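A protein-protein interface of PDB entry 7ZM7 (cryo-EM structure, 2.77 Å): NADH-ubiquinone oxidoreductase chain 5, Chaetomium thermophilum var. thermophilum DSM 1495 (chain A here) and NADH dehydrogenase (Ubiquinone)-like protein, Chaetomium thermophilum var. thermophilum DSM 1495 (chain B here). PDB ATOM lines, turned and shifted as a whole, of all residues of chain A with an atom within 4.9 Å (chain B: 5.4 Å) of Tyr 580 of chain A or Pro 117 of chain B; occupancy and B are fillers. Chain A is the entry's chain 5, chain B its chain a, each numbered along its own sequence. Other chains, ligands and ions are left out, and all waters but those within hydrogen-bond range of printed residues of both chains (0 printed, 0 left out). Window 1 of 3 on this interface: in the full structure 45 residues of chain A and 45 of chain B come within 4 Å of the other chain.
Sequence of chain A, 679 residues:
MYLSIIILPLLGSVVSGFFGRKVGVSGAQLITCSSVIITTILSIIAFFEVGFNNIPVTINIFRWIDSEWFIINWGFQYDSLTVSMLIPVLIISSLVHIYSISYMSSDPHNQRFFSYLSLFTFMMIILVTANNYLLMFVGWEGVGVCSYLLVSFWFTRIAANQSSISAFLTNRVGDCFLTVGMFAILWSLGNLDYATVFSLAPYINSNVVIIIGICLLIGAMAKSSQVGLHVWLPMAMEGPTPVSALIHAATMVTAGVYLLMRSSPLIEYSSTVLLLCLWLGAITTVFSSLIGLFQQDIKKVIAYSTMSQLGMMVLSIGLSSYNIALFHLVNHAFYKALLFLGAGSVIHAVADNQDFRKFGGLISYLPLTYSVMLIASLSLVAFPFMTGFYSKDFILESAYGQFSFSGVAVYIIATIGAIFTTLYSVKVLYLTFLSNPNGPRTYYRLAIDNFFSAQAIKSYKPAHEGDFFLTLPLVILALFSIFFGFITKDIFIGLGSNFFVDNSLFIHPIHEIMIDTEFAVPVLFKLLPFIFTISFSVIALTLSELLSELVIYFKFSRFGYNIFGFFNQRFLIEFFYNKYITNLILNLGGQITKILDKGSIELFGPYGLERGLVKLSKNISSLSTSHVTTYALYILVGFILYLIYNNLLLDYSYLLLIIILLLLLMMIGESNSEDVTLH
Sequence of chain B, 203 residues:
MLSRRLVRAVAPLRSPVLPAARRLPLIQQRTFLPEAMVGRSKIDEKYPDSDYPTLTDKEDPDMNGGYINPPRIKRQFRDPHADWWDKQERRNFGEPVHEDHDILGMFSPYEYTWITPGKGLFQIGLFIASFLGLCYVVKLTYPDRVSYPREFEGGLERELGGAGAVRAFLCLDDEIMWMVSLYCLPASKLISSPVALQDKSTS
Printed residues of chain B within 4 Å of Tyr 580 of chain A: Pro 117 (3.8 Å). Of chain A, only Phe 575, Phe 576 and Tyr 580 come within 4 Å of Pro 117 of chain B. Printed residues of chain B within 4 Å of Phe 575 of chain A: Pro 117 (3.6 Å). Printed residues of chain B within 4 Å of Phe 576 of chain A: Pro 117 (3.7 Å) and Leu 121 (3.8 Å). The nearest printed residue of chain B that does not touch Tyr 580 of chain A is Gly 118 of chain B (5.7 Å). The nearest residue of chain A that does not touch Pro 117 of chain B is Lys 579 of chain A (4.4 Å). The nearest printed residue of chain A that does not touch Leu 121 of chain B is Phe 575 of chain A (6.6 Å).
Phe 575 of chain A touches Pro 117 of chain B (CZ to CA, 3.6 Å). O of Pro 117 of chain B touches CZ of Phe 576 of chain A (3.7 Å). Phe 576 of chain A touches Leu 121 of chain B (CZ to N, 3.8 Å). OH of Tyr 580 of chain A touches CB of Pro 117 of chain B, 3.8 Å away.
Hydrophobic or aromatic side chains of chain A that line the printed part of chain B: Phe 575, Phe 576 and Tyr 580. Hydrophobic or aromatic side chains of chain B that line the printed part of chain A: Pro 117. Among the printed residues, 4 pairs touch across the chains.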
ATOM      1  N   PHE A 575      28.908  30.816  33.362  1.00  0.00           N
ATOM      2  CA  PHE A 575      28.379  30.819  32.008  1.00  0.00           C
ATOM      3  C   PHE A 575      28.641  29.490  31.316  1.00  0.00           C
ATOM      4  O   PHE A 575      27.750  28.929  30.665  1.00  0.00           O
ATOM      5  CB  PHE A 575      29.003  31.969  31.224  1.00  0.00           C
ATOM      6  CG  PHE A 575      28.872  31.839  29.750  1.00  0.00           C
ATOM      7  CD1 PHE A 575      27.692  32.161  29.115  1.00  0.00           C
ATOM      8  CD2 PHE A 575      29.932  31.389  28.991  1.00  0.00           C
ATOM      9  CE1 PHE A 575      27.573  32.040  27.749  1.00  0.00           C
ATOM     10  CE2 PHE A 575      29.822  31.265  27.632  1.00  0.00           C
ATOM     11  CZ  PHE A 575      28.642  31.591  27.006  1.00  0.00           C
ATOM     12  N   PHE A 576      29.857  28.963  31.452  1.00  0.00           N
ATOM     13  CA  PHE A 576      30.207  27.725  30.769  1.00  0.00           C
ATOM     14  C   PHE A 576      29.574  26.517  31.446  1.00  0.00           C
ATOM     15  O   PHE A 576      29.049  25.626  30.774  1.00  0.00           O
ATOM     16  CB  PHE A 576      31.721  27.580  30.708  1.00  0.00           C
ATOM     17  CG  PHE A 576      32.318  28.127  29.457  1.00  0.00           C
ATOM     18  CD1 PHE A 576      31.938  27.637  28.222  1.00  0.00           C
ATOM     19  CD2 PHE A 576      33.231  29.155  29.508  1.00  0.00           C
ATOM     20  CE1 PHE A 576      32.479  28.149  27.079  1.00  0.00           C
ATOM     21  CE2 PHE A 576      33.774  29.658  28.367  1.00  0.00           C
ATOM     22  CZ  PHE A 576      33.396  29.158  27.152  1.00  0.00           C
ATOM     23  N   TYR A 577      29.617  26.463  32.776  1.00  0.00           N
ATOM     24  CA  TYR A 577      28.966  25.362  33.476  1.00  0.00           C
ATOM     25  C   TYR A 577      27.480  25.343  33.192  1.00  0.00           C
ATOM     26  O   TYR A 577      26.888  24.283  32.981  1.00  0.00           O
ATOM     27  CB  TYR A 577      29.172  25.479  34.980  1.00  0.00           C
ATOM     28  CG  TYR A 577      30.496  25.018  35.490  1.00  0.00           C
ATOM     29  CD1 TYR A 577      31.519  24.679  34.630  1.00  0.00           C
ATOM     30  CD2 TYR A 577      30.731  24.947  36.839  1.00  0.00           C
ATOM     31  CE1 TYR A 577      32.728  24.277  35.111  1.00  0.00           C
ATOM     32  CE2 TYR A 577      31.929  24.543  37.319  1.00  0.00           C
ATOM     33  CZ  TYR A 577      32.923  24.218  36.462  1.00  0.00           C
ATOM     34  OH  TYR A 577      34.114  23.813  36.989  1.00  0.00           O
ATOM     35  N   ASN A 578      26.818  26.465  33.286  1.00  0.00           N
ATOM     36  CA  ASN A 578      25.334  26.540  33.170  1.00  0.00           C
ATOM     37  C   ASN A 578      24.890  26.176  31.768  1.00  0.00           C
ATOM     38  O   ASN A 578      23.872  25.510  31.636  1.00  0.00           O
ATOM     39  CB  ASN A 578      24.828  27.935  33.518  1.00  0.00           C
ATOM     40  CG  ASN A 578      23.737  27.964  34.563  1.00  0.00           C
ATOM     41  OD1 ASN A 578      23.362  26.932  35.111  1.00  0.00           O
ATOM     42  ND2 ASN A 578      23.222  29.146  34.842  1.00  0.00           N
ATOM     43  N   LYS A 579      25.686  26.566  30.766  1.00  0.00           N
ATOM     44  CA  LYS A 579      25.313  26.330  29.376  1.00  0.00           C
ATOM     45  C   LYS A 579      25.763  24.984  28.841  1.00  0.00           C
ATOM     46  O   LYS A 579      25.031  24.355  28.073  1.00  0.00           O
ATOM     47  CB  LYS A 579      25.908  27.415  28.475  1.00  0.00           C
ATOM     48  CG  LYS A 579      25.302  27.467  27.090  1.00  0.00           C
ATOM     49  CD  LYS A 579      26.010  28.478  26.219  1.00  0.00           C
ATOM     50  CE  LYS A 579      25.228  28.750  24.948  1.00  0.00           C
ATOM     51  NZ  LYS A 579      23.921  29.393  25.241  1.00  0.00           N
ATOM     52  N   TYR A 580      26.960  24.546  29.201  1.00  0.00           N
ATOM     53  CA  TYR A 580      27.543  23.344  28.628  1.00  0.00           C
ATOM     54  C   TYR A 580      27.313  22.116  29.483  1.00  0.00           C
ATOM     55  O   TYR A 580      27.145  21.022  28.943  1.00  0.00           O
ATOM     56  CB  TYR A 580      29.048  23.547  28.410  1.00  0.00           C
ATOM     57  CG  TYR A 580      29.380  24.317  27.161  1.00  0.00           C
ATOM     58  CD1 TYR A 580      28.608  25.389  26.762  1.00  0.00           C
ATOM     59  CD2 TYR A 580      30.458  23.966  26.377  1.00  0.00           C
ATOM     60  CE1 TYR A 580      28.897  26.086  25.623  1.00  0.00           C
ATOM     61  CE2 TYR A 580      30.756  24.656  25.235  1.00  0.00           C
ATOM     62  CZ  TYR A 580      29.970  25.716  24.862  1.00  0.00           C
ATOM     63  OH  TYR A 580      30.266  26.419  23.718  1.00  0.00           O
ATOM     64  N   ILE A 581      27.264  22.275  30.796  1.00  0.00           N
ATOM     65  CA  ILE A 581      27.121  21.164  31.725  1.00  0.00           C
ATOM     66  C   ILE A 581      25.687  21.037  32.210  1.00  0.00           C
ATOM     67  O   ILE A 581      25.063  19.990  32.053  1.00  0.00           O
ATOM     68  CB  ILE A 581      28.101  21.305  32.908  1.00  0.00           C
ATOM     69  CG1 ILE A 581      29.488  21.686  32.389  1.00  0.00           C
ATOM     70  CG2 ILE A 581      28.102  20.054  33.759  1.00  0.00           C
ATOM     71  CD1 ILE A 581      30.115  20.638  31.540  1.00  0.00           C
ATOM     72  N   THR A 582      25.139  22.105  32.791  1.00  0.00           N
ATOM     73  CA  THR A 582      23.812  22.027  33.390  1.00  0.00           C
ATOM     74  C   THR A 582      22.736  21.860  32.335  1.00  0.00           C
ATOM     75  O   THR A 582      21.865  20.994  32.458  1.00  0.00           O
ATOM     76  CB  THR A 582      23.536  23.269  34.229  1.00  0.00           C
ATOM     77  OG1 THR A 582      24.497  23.352  35.285  1.00  0.00           O
ATOM     78  CG2 THR A 582      22.164  23.192  34.829  1.00  0.00           C
ATOM     79  N   LEU A 584      23.126  20.829  29.303  1.00  0.00           N
ATOM     80  CA  LEU A 584      23.277  19.562  28.605  1.00  0.00           C
ATOM     81  C   LEU A 584      22.508  18.461  29.315  1.00  0.00           C
ATOM     82  O   LEU A 584      21.869  17.624  28.670  1.00  0.00           O
ATOM     83  CB  LEU A 584      24.753  19.203  28.484  1.00  0.00           C
ATOM     84  CG  LEU A 584      25.117  17.731  28.306  1.00  0.00           C
ATOM     85  CD1 LEU A 584      24.734  17.224  26.935  1.00  0.00           C
ATOM     86  CD2 LEU A 584      26.597  17.517  28.565  1.00  0.00           C
ATOM     87  N   ILE B 115      29.088  37.714  26.899  1.00  0.00           N
ATOM     88  CA  ILE B 115      29.766  37.535  25.626  1.00  0.00           C
ATOM     89  C   ILE B 115      29.302  36.235  24.986  1.00  0.00           C
ATOM     90  O   ILE B 115      28.700  35.375  25.627  1.00  0.00           O
ATOM     91  CB  ILE B 115      31.303  37.531  25.760  1.00  0.00           C
ATOM     92  CG1 ILE B 115      31.760  36.495  26.773  1.00  0.00           C
ATOM     93  CG2 ILE B 115      31.833  38.905  26.145  1.00  0.00           C
ATOM     94  CD1 ILE B 115      33.214  36.180  26.610  1.00  0.00           C
ATOM     95  N   THR B 116      29.582  36.112  23.695  1.00  0.00           N
ATOM     96  CA  THR B 116      29.319  34.886  22.959  1.00  0.00           C
ATOM     97  C   THR B 116      30.221  33.772  23.486  1.00  0.00           C
ATOM     98  O   THR B 116      31.344  34.043  23.921  1.00  0.00           O
ATOM     99  CB  THR B 116      29.564  35.143  21.466  1.00  0.00           C
ATOM    100  OG1 THR B 116      28.540  36.010  20.962  1.00  0.00           O
ATOM    101  CG2 THR B 116      29.584  33.864  20.646  1.00  0.00           C
ATOM    102  N   PRO B 117      29.751  32.520  23.510  1.00  0.00           N
ATOM    103  CA  PRO B 117      30.607  31.433  24.014  1.00  0.00           C
ATOM    104  C   PRO B 117      31.907  31.268  23.257  1.00  0.00           C
ATOM    105  O   PRO B 117      32.914  30.885  23.860  1.00  0.00           O
ATOM    106  CB  PRO B 117      29.713  30.194  23.872  1.00  0.00           C
ATOM    107  CG  PRO B 117      28.645  30.589  22.916  1.00  0.00           C
ATOM    108  CD  PRO B 117      28.401  32.034  23.190  1.00  0.00           C
ATOM    109  N   GLY B 118      31.917  31.534  21.952  1.00  0.00           N
ATOM    110  CA  GLY B 118      33.154  31.412  21.201  1.00  0.00           C
ATOM    111  C   GLY B 118      34.235  32.344  21.708  1.00  0.00           C
ATOM    112  O   GLY B 118      35.395  31.950  21.846  1.00  0.00           O
ATOM    113  N   LYS B 119      33.868  33.592  22.006  1.00  0.00           N
ATOM    114  CA  LYS B 119      34.859  34.557  22.464  1.00  0.00           C
ATOM    115  C   LYS B 119      35.377  34.207  23.849  1.00  0.00           C
ATOM    116  O   LYS B 119      36.538  34.490  24.164  1.00  0.00           O
ATOM    117  CB  LYS B 119      34.260  35.962  22.453  1.00  0.00           C
ATOM    118  CG  LYS B 119      35.270  37.066  22.225  1.00  0.00           C
ATOM    119  CD  LYS B 119      34.586  38.341  21.765  1.00  0.00           C
ATOM    120  CE  LYS B 119      34.345  39.292  22.921  1.00  0.00           C
ATOM    121  NZ  LYS B 119      33.654  40.529  22.472  1.00  0.00           N
ATOM    122  N   GLY B 120      34.532  33.600  24.683  1.00  0.00           N
ATOM    123  CA  GLY B 120      34.951  33.246  26.026  1.00  0.00           C
ATOM    124  C   GLY B 120      36.048  32.206  26.045  1.00  0.00           C
ATOM    125  O   GLY B 120      37.001  32.311  26.818  1.00  0.00           O
ATOM    126  N   LEU B 121      35.932  31.188  25.196  1.00  0.00           N
ATOM    127  CA  LEU B 121      36.992  30.200  25.091  1.00  0.00           C
ATOM    128  C   LEU B 121      38.315  30.851  24.724  1.00  0.00           C
ATOM    129  O   LEU B 121      39.375  30.405  25.175  1.00  0.00           O
ATOM    130  CB  LEU B 121      36.614  29.139  24.065  1.00  0.00           C
ATOM    131  CG  LEU B 121      37.599  27.982  23.908  1.00  0.00           C
ATOM    132  CD1 LEU B 121      37.706  27.206  25.204  1.00  0.00           C
ATOM    133  CD2 LEU B 121      37.169  27.071  22.774  1.00  0.00           C
